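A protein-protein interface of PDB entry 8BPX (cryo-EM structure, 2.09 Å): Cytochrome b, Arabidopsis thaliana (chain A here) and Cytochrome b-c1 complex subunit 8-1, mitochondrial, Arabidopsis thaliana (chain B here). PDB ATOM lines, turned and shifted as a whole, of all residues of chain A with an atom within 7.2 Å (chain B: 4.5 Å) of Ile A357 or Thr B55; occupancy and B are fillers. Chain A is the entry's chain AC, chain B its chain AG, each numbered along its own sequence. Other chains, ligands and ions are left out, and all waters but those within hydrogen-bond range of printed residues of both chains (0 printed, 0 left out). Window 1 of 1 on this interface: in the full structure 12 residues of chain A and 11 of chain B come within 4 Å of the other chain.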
ATOM      1  N   SER A 290     -10.308  12.859   3.017  1.00  0.00           N
ATOM      2  CA  SER A 290     -11.176  12.878   4.189  1.00  0.00           C
ATOM      3  C   SER A 290     -10.667  11.973   5.303  1.00  0.00           C
ATOM      4  O   SER A 290     -11.075  12.140   6.455  1.00  0.00           O
ATOM      5  CB  SER A 290     -12.600  12.477   3.803  1.00  0.00           C
ATOM      6  OG  SER A 290     -12.643  11.143   3.336  1.00  0.00           O
ATOM      7  N   ASP A 338     -24.461  14.337  -3.120  1.00  0.00           N
ATOM      8  CA  ASP A 338     -23.262  14.062  -2.343  1.00  0.00           C
ATOM      9  C   ASP A 338     -22.033  13.917  -3.237  1.00  0.00           C
ATOM     10  O   ASP A 338     -20.944  14.383  -2.888  1.00  0.00           O
ATOM     11  CB  ASP A 338     -23.483  12.805  -1.508  1.00  0.00           C
ATOM     12  CG  ASP A 338     -22.477  12.658  -0.399  1.00  0.00           C
ATOM     13  OD1 ASP A 338     -22.184  13.661   0.280  1.00  0.00           O
ATOM     14  OD2 ASP A 338     -21.987  11.531  -0.209  1.00  0.00           O
ATOM     15  N   LEU A 341     -20.987  17.299  -4.375  1.00  0.00           N
ATOM     16  CA  LEU A 341     -20.325  17.965  -3.258  1.00  0.00           C
ATOM     17  C   LEU A 341     -18.900  17.457  -3.073  1.00  0.00           C
ATOM     18  O   LEU A 341     -17.991  18.241  -2.787  1.00  0.00           O
ATOM     19  CB  LEU A 341     -21.136  17.762  -1.977  1.00  0.00           C
ATOM     20  CG  LEU A 341     -22.314  18.705  -1.713  1.00  0.00           C
ATOM     21  CD1 LEU A 341     -22.718  18.654  -0.251  1.00  0.00           C
ATOM     22  CD2 LEU A 341     -21.981  20.131  -2.120  1.00  0.00           C
ATOM     23  N   LEU A 342     -18.690  16.147  -3.206  1.00  0.00           N
ATOM     24  CA  LEU A 342     -17.339  15.602  -3.081  1.00  0.00           C
ATOM     25  C   LEU A 342     -16.430  16.155  -4.168  1.00  0.00           C
ATOM     26  O   LEU A 342     -15.273  16.505  -3.907  1.00  0.00           O
ATOM     27  CB  LEU A 342     -17.376  14.076  -3.132  1.00  0.00           C
ATOM     28  CG  LEU A 342     -17.758  13.384  -1.821  1.00  0.00           C
ATOM     29  CD1 LEU A 342     -18.180  11.944  -2.070  1.00  0.00           C
ATOM     30  CD2 LEU A 342     -16.629  13.458  -0.804  1.00  0.00           C
ATOM     31  N   TRP A 344     -16.750  19.087  -5.672  1.00  0.00           N
ATOM     32  CA  TRP A 344     -16.458  20.478  -5.336  1.00  0.00           C
ATOM     33  C   TRP A 344     -15.451  20.574  -4.193  1.00  0.00           C
ATOM     34  O   TRP A 344     -14.575  21.445  -4.203  1.00  0.00           O
ATOM     35  CB  TRP A 344     -17.749  21.218  -4.983  1.00  0.00           C
ATOM     36  CG  TRP A 344     -17.542  22.552  -4.324  1.00  0.00           C
ATOM     37  CD1 TRP A 344     -17.099  23.698  -4.913  1.00  0.00           C
ATOM     38  CD2 TRP A 344     -17.780  22.875  -2.949  1.00  0.00           C
ATOM     39  NE1 TRP A 344     -17.042  24.713  -3.993  1.00  0.00           N
ATOM     40  CE2 TRP A 344     -17.457  24.234  -2.779  1.00  0.00           C
ATOM     41  CE3 TRP A 344     -18.236  22.146  -1.848  1.00  0.00           C
ATOM     42  CZ2 TRP A 344     -17.574  24.882  -1.552  1.00  0.00           C
ATOM     43  CZ3 TRP A 344     -18.350  22.791  -0.628  1.00  0.00           C
ATOM     44  CH2 TRP A 344     -18.019  24.144  -0.491  1.00  0.00           C
ATOM     45  N   ILE A 345     -15.560  19.685  -3.202  1.00  0.00           N
ATOM     46  CA  ILE A 345     -14.664  19.713  -2.051  1.00  0.00           C
ATOM     47  C   ILE A 345     -13.238  19.369  -2.471  1.00  0.00           C
ATOM     48  O   ILE A 345     -12.273  19.962  -1.976  1.00  0.00           O
ATOM     49  CB  ILE A 345     -15.179  18.763  -0.951  1.00  0.00           C
ATOM     50  CG1 ILE A 345     -16.382  19.376  -0.230  1.00  0.00           C
ATOM     51  CG2 ILE A 345     -14.081  18.436   0.047  1.00  0.00           C
ATOM     52  CD1 ILE A 345     -16.025  20.510   0.709  1.00  0.00           C
ATOM     53  N   ALA A 352     -10.396  24.150   7.280  1.00  0.00           N
ATOM     54  CA  ALA A 352     -11.768  24.314   7.735  1.00  0.00           C
ATOM     55  C   ALA A 352     -12.530  25.240   6.789  1.00  0.00           C
ATOM     56  O   ALA A 352     -11.950  26.188   6.246  1.00  0.00           O
ATOM     57  CB  ALA A 352     -11.800  24.874   9.155  1.00  0.00           C
ATOM     58  N   PRO A 353     -13.826  24.996   6.559  1.00  0.00           N
ATOM     59  CA  PRO A 353     -14.665  23.936   7.126  1.00  0.00           C
ATOM     60  C   PRO A 353     -14.658  22.671   6.276  1.00  0.00           C
ATOM     61  O   PRO A 353     -15.451  21.764   6.501  1.00  0.00           O
ATOM     62  CB  PRO A 353     -16.057  24.580   7.133  1.00  0.00           C
ATOM     63  CG  PRO A 353     -16.014  25.666   6.050  1.00  0.00           C
ATOM     64  CD  PRO A 353     -14.581  25.780   5.571  1.00  0.00           C
ATOM     65  N   PHE A 354     -13.768  22.592   5.287  1.00  0.00           N
ATOM     66  CA  PHE A 354     -13.888  21.575   4.251  1.00  0.00           C
ATOM     67  C   PHE A 354     -13.473  20.182   4.707  1.00  0.00           C
ATOM     68  O   PHE A 354     -13.888  19.203   4.080  1.00  0.00           O
ATOM     69  CB  PHE A 354     -13.083  21.993   3.025  1.00  0.00           C
ATOM     70  CG  PHE A 354     -13.489  23.322   2.471  1.00  0.00           C
ATOM     71  CD1 PHE A 354     -14.792  23.542   2.056  1.00  0.00           C
ATOM     72  CD2 PHE A 354     -12.576  24.354   2.365  1.00  0.00           C
ATOM     73  CE1 PHE A 354     -15.171  24.762   1.544  1.00  0.00           C
ATOM     74  CE2 PHE A 354     -12.950  25.576   1.855  1.00  0.00           C
ATOM     75  CZ  PHE A 354     -14.251  25.781   1.444  1.00  0.00           C
ATOM     76  N   VAL A 355     -12.691  20.058   5.778  1.00  0.00           N
ATOM     77  CA  VAL A 355     -12.350  18.733   6.290  1.00  0.00           C
ATOM     78  C   VAL A 355     -13.592  18.040   6.841  1.00  0.00           C
ATOM     79  O   VAL A 355     -13.865  16.875   6.529  1.00  0.00           O
ATOM     80  CB  VAL A 355     -11.237  18.834   7.349  1.00  0.00           C
ATOM     81  CG1 VAL A 355     -10.779  17.450   7.778  1.00  0.00           C
ATOM     82  CG2 VAL A 355     -10.070  19.634   6.804  1.00  0.00           C
ATOM     83  N   THR A 356     -14.367  18.754   7.662  1.00  0.00           N
ATOM     84  CA  THR A 356     -15.599  18.190   8.208  1.00  0.00           C
ATOM     85  C   THR A 356     -16.603  17.878   7.106  1.00  0.00           C
ATOM     86  O   THR A 356     -17.242  16.817   7.116  1.00  0.00           O
ATOM     87  CB  THR A 356     -16.207  19.157   9.226  1.00  0.00           C
ATOM     88  OG1 THR A 356     -15.229  19.477  10.222  1.00  0.00           O
ATOM     89  CG2 THR A 356     -17.422  18.545   9.897  1.00  0.00           C
ATOM     90  N   ILE A 357     -16.760  18.794   6.151  1.00  0.00           N
ATOM     91  CA  ILE A 357     -17.707  18.586   5.063  1.00  0.00           C
ATOM     92  C   ILE A 357     -17.296  17.383   4.223  1.00  0.00           C
ATOM     93  O   ILE A 357     -18.134  16.557   3.846  1.00  0.00           O
ATOM     94  CB  ILE A 357     -17.841  19.865   4.216  1.00  0.00           C
ATOM     95  CG1 ILE A 357     -18.423  21.000   5.065  1.00  0.00           C
ATOM     96  CG2 ILE A 357     -18.724  19.616   3.004  1.00  0.00           C
ATOM     97  CD1 ILE A 357     -18.315  22.362   4.431  1.00  0.00           C
ATOM     98  N   GLY A 358     -15.997  17.254   3.938  1.00  0.00           N
ATOM     99  CA  GLY A 358     -15.522  16.100   3.195  1.00  0.00           C
ATOM    100  C   GLY A 358     -15.736  14.797   3.938  1.00  0.00           C
ATOM    101  O   GLY A 358     -16.126  13.791   3.342  1.00  0.00           O
ATOM    102  N   GLN A 359     -15.489  14.797   5.249  1.00  0.00           N
ATOM    103  CA  GLN A 359     -15.698  13.592   6.044  1.00  0.00           C
ATOM    104  C   GLN A 359     -17.164  13.170   6.025  1.00  0.00           C
ATOM    105  O   GLN A 359     -17.485  11.994   5.800  1.00  0.00           O
ATOM    106  CB  GLN A 359     -15.217  13.830   7.476  1.00  0.00           C
ATOM    107  CG  GLN A 359     -13.829  13.294   7.760  1.00  0.00           C
ATOM    108  CD  GLN A 359     -13.056  14.149   8.750  1.00  0.00           C
ATOM    109  OE1 GLN A 359     -13.627  14.991   9.441  1.00  0.00           O
ATOM    110  NE2 GLN A 359     -11.749  13.933   8.821  1.00  0.00           N
ATOM    111  N   ILE A 360     -18.069  14.126   6.236  1.00  0.00           N
ATOM    112  CA  ILE A 360     -19.495  13.810   6.238  1.00  0.00           C
ATOM    113  C   ILE A 360     -19.946  13.344   4.857  1.00  0.00           C
ATOM    114  O   ILE A 360     -20.747  12.407   4.737  1.00  0.00           O
ATOM    115  CB  ILE A 360     -20.308  15.018   6.737  1.00  0.00           C
ATOM    116  CG1 ILE A 360     -20.057  15.238   8.227  1.00  0.00           C
ATOM    117  CG2 ILE A 360     -21.798  14.825   6.471  1.00  0.00           C
ATOM    118  CD1 ILE A 360     -20.335  16.643   8.685  1.00  0.00           C
ATOM    119  N   SER A 361     -19.443  13.982   3.797  1.00  0.00           N
ATOM    120  CA  SER A 361     -19.811  13.575   2.445  1.00  0.00           C
ATOM    121  C   SER A 361     -19.332  12.159   2.140  1.00  0.00           C
ATOM    122  O   SER A 361     -20.069  11.365   1.546  1.00  0.00           O
ATOM    123  CB  SER A 361     -19.250  14.566   1.428  1.00  0.00           C
ATOM    124  OG  SER A 361     -19.961  15.788   1.459  1.00  0.00           O
ATOM    125  N   SER A 362     -18.102  11.823   2.536  1.00  0.00           N
ATOM    126  CA  SER A 362     -17.615  10.459   2.344  1.00  0.00           C
ATOM    127  C   SER A 362     -18.480   9.459   3.098  1.00  0.00           C
ATOM    128  O   SER A 362     -18.810   8.381   2.578  1.00  0.00           O
ATOM    129  CB  SER A 362     -16.158  10.358   2.796  1.00  0.00           C
ATOM    130  OG  SER A 362     -15.359  11.343   2.173  1.00  0.00           O
ATOM    131  N   LEU A 363     -18.867   9.810   4.328  1.00  0.00           N
ATOM    132  CA  LEU A 363     -19.748   8.939   5.097  1.00  0.00           C
ATOM    133  C   LEU A 363     -21.078   8.725   4.382  1.00  0.00           C
ATOM    134  O   LEU A 363     -21.571   7.596   4.311  1.00  0.00           O
ATOM    135  CB  LEU A 363     -19.970   9.524   6.490  1.00  0.00           C
ATOM    136  CG  LEU A 363     -20.991   8.814   7.377  1.00  0.00           C
ATOM    137  CD1 LEU A 363     -20.671   7.336   7.507  1.00  0.00           C
ATOM    138  CD2 LEU A 363     -21.048   9.473   8.739  1.00  0.00           C
ATOM    139  N   PRO B  51     -29.156  20.132  -0.621  1.00  0.00           N
ATOM    140  CA  PRO B  51     -27.861  19.871   0.029  1.00  0.00           C
ATOM    141  C   PRO B  51     -26.711  20.634  -0.606  1.00  0.00           C
ATOM    142  O   PRO B  51     -25.888  21.207   0.117  1.00  0.00           O
ATOM    143  CB  PRO B  51     -27.690  18.351  -0.120  1.00  0.00           C
ATOM    144  CG  PRO B  51     -29.064  17.834  -0.327  1.00  0.00           C
ATOM    145  CD  PRO B  51     -29.768  18.885  -1.114  1.00  0.00           C
ATOM    146  N   VAL B  52     -26.660  20.695  -1.937  1.00  0.00           N
ATOM    147  CA  VAL B  52     -25.554  21.363  -2.620  1.00  0.00           C
ATOM    148  C   VAL B  52     -25.534  22.851  -2.286  1.00  0.00           C
ATOM    149  O   VAL B  52     -24.505  23.397  -1.867  1.00  0.00           O
ATOM    150  CB  VAL B  52     -25.644  21.136  -4.140  1.00  0.00           C
ATOM    151  CG1 VAL B  52     -24.525  21.873  -4.846  1.00  0.00           C
ATOM    152  CG2 VAL B  52     -25.595  19.651  -4.467  1.00  0.00           C
ATOM    153  N   VAL B  53     -26.674  23.521  -2.454  1.00  0.00           N
ATOM    154  CA  VAL B  53     -26.726  24.964  -2.232  1.00  0.00           C
ATOM    155  C   VAL B  53     -26.530  25.286  -0.759  1.00  0.00           C
ATOM    156  O   VAL B  53     -25.836  26.248  -0.410  1.00  0.00           O
ATOM    157  CB  VAL B  53     -28.042  25.547  -2.776  1.00  0.00           C
ATOM    158  CG1 VAL B  53     -28.199  26.997  -2.349  1.00  0.00           C
ATOM    159  CG2 VAL B  53     -28.081  25.436  -4.290  1.00  0.00           C
ATOM    160  N   GLY B  54     -27.131  24.492   0.129  1.00  0.00           N
ATOM    161  CA  GLY B  54     -26.949  24.721   1.551  1.00  0.00           C
ATOM    162  C   GLY B  54     -25.503  24.579   1.983  1.00  0.00           C
ATOM    163  O   GLY B  54     -24.980  25.412   2.725  1.00  0.00           O
ATOM    164  N   THR B  55     -24.833  23.523   1.514  1.00  0.00           N
ATOM    165  CA  THR B  55     -23.433  23.320   1.867  1.00  0.00           C
ATOM    166  C   THR B  55     -22.554  24.426   1.300  1.00  0.00           C
ATOM    167  O   THR B  55     -21.662  24.930   1.989  1.00  0.00           O
ATOM    168  CB  THR B  55     -22.966  21.948   1.380  1.00  0.00           C
ATOM    169  OG1 THR B  55     -23.887  20.949   1.832  1.00  0.00           O
ATOM    170  CG2 THR B  55     -21.585  21.629   1.920  1.00  0.00           C
ATOM    171  N   TYR B  56     -22.808  24.832   0.053  1.00  0.00           N
ATOM    172  CA  TYR B  56     -22.041  25.922  -0.537  1.00  0.00           C
ATOM    173  C   TYR B  56     -22.219  27.210   0.259  1.00  0.00           C
ATOM    174  O   TYR B  56     -21.238  27.886   0.596  1.00  0.00           O
ATOM    175  CB  TYR B  56     -22.458  26.123  -1.993  1.00  0.00           C
ATOM    176  CG  TYR B  56     -21.636  27.159  -2.713  1.00  0.00           C
ATOM    177  CD1 TYR B  56     -20.419  26.823  -3.291  1.00  0.00           C
ATOM    178  CD2 TYR B  56     -22.066  28.475  -2.805  1.00  0.00           C
ATOM    179  CE1 TYR B  56     -19.658  27.766  -3.945  1.00  0.00           C
ATOM    180  CE2 TYR B  56     -21.310  29.424  -3.455  1.00  0.00           C
ATOM    181  CZ  TYR B  56     -20.107  29.065  -4.022  1.00  0.00           C
ATOM    182  OH  TYR B  56     -19.351  30.008  -4.674  1.00  0.00           O
ATOM    183  N   TRP B  57     -23.469  27.555   0.581  1.00  0.00           N
ATOM    184  CA  TRP B  57     -23.739  28.782   1.321  1.00  0.00           C
ATOM    185  C   TRP B  57     -23.096  28.744   2.698  1.00  0.00           C
ATOM    186  O   TRP B  57     -22.521  29.743   3.147  1.00  0.00           O
ATOM    187  CB  TRP B  57     -25.247  29.008   1.440  1.00  0.00           C
ATOM    188  CG  TRP B  57     -25.621  30.438   1.690  1.00  0.00           C
ATOM    189  CD1 TRP B  57     -25.973  31.368   0.754  1.00  0.00           C
ATOM    190  CD2 TRP B  57     -25.679  31.104   2.958  1.00  0.00           C
ATOM    191  NE1 TRP B  57     -26.246  32.569   1.360  1.00  0.00           N
ATOM    192  CE2 TRP B  57     -26.074  32.433   2.711  1.00  0.00           C
ATOM    193  CE3 TRP B  57     -25.438  30.704   4.276  1.00  0.00           C
ATOM    194  CZ2 TRP B  57     -26.231  33.367   3.735  1.00  0.00           C
ATOM    195  CZ3 TRP B  57     -25.591  31.630   5.288  1.00  0.00           C
ATOM    196  CH2 TRP B  57     -25.985  32.946   5.013  1.00  0.00           C
ATOM    197  N   TYR B  58     -23.178  27.601   3.383  1.00  0.00           N
ATOM    198  CA  TYR B  58     -22.565  27.501   4.701  1.00  0.00           C
ATOM    199  C   TYR B  58     -21.052  27.645   4.612  1.00  0.00           C
ATOM    200  O   TYR B  58     -20.433  28.267   5.480  1.00  0.00           O
ATOM    201  CB  TYR B  58     -22.940  26.179   5.372  1.00  0.00           C
ATOM    202  CG  TYR B  58     -22.061  25.855   6.556  1.00  0.00           C
ATOM    203  CD1 TYR B  58     -22.287  26.442   7.793  1.00  0.00           C
ATOM    204  CD2 TYR B  58     -20.992  24.978   6.435  1.00  0.00           C
ATOM    205  CE1 TYR B  58     -21.480  26.162   8.876  1.00  0.00           C
ATOM    206  CE2 TYR B  58     -20.181  24.693   7.508  1.00  0.00           C
ATOM    207  CZ  TYR B  58     -20.428  25.286   8.727  1.00  0.00           C
ATOM    208  OH  TYR B  58     -19.619  24.997   9.798  1.00  0.00           O
ATOM    209  N   ALA B  59     -20.436  27.064   3.578  1.00  0.00           N
ATOM    210  CA  ALA B  59     -18.990  27.192   3.423  1.00  0.00           C
ATOM    211  C   ALA B  59     -18.578  28.641   3.186  1.00  0.00           C
ATOM    212  O   ALA B  59     -17.605  29.118   3.781  1.00  0.00           O
ATOM    213  CB  ALA B  59     -18.496  26.300   2.284  1.00  0.00           C
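Of the 18 printed residues of chain A, 4 touch a printed residue of chain B. Printed residues of chain A that touch a printed residue of chain B: Leu A341, Trp A344, Phe A354 and Ile A357. Hydrophobic or aromatic side chains of chain A within 4 Å of the printed part of chain B: Leu A341, Trp A344, Phe A354 and Ile A357. Hydrophobic or aromatic side chains of chain B within 4 Å of the printed part of chain A: Tyr B56 and Ala B59. Among the printed residues, 6 pairs touch across the chains. Among the printed residues, no Asp or Glu carboxylate lies within 4 Å of a Lys or Arg side-chain nitrogen of the other chain.
Ile A357 touches just one residue of chain B: Thr B55 (3.7 Å). Thr B55 touches just these residues of chain A: Leu A341 and Ile A357. No residue of chain A comes within 4 Å of Gly B54. Printed residues of chain B within 4 Å of Phe A354: Ala B59 (3.7 Å). Of the printed residues of chain B, Leu A341 touches Val B52 (3.8 Å) and Thr B55 (3.3 Å). Printed residues of chain A within 4 Å of Tyr B56: Trp A344. Leu A342 touches none of the printed residues of chain B. Asp A338 touches none of the printed residues of chain B. The nearest printed residue of chain B that does not touch Phe A354 is Thr B55 (6.5 Å).
CD2 of Leu A341 touches CA of Val B52, 3.8 Å away. Leu A341 touches Thr B55 (CD1 to OG1, 3.3 Å). Trp A344 touches Tyr B56. Ala B59 touches Trp A344 (CB to CH2, 3.5 Å). Ala B59 touches Phe A354. Ile A357 touches Thr B55 (CG2 to CG2, 3.7 Å).
The backbone carbonyl oxygen (O) of Ile A357 lies within hydrogen-bond range of the side-chain hydroxyl (OG) of Ser A361 (3.1 Å). OG1 of Thr B55 lies within hydrogen-bond range of O of Pro B51, at 2.6 Å.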
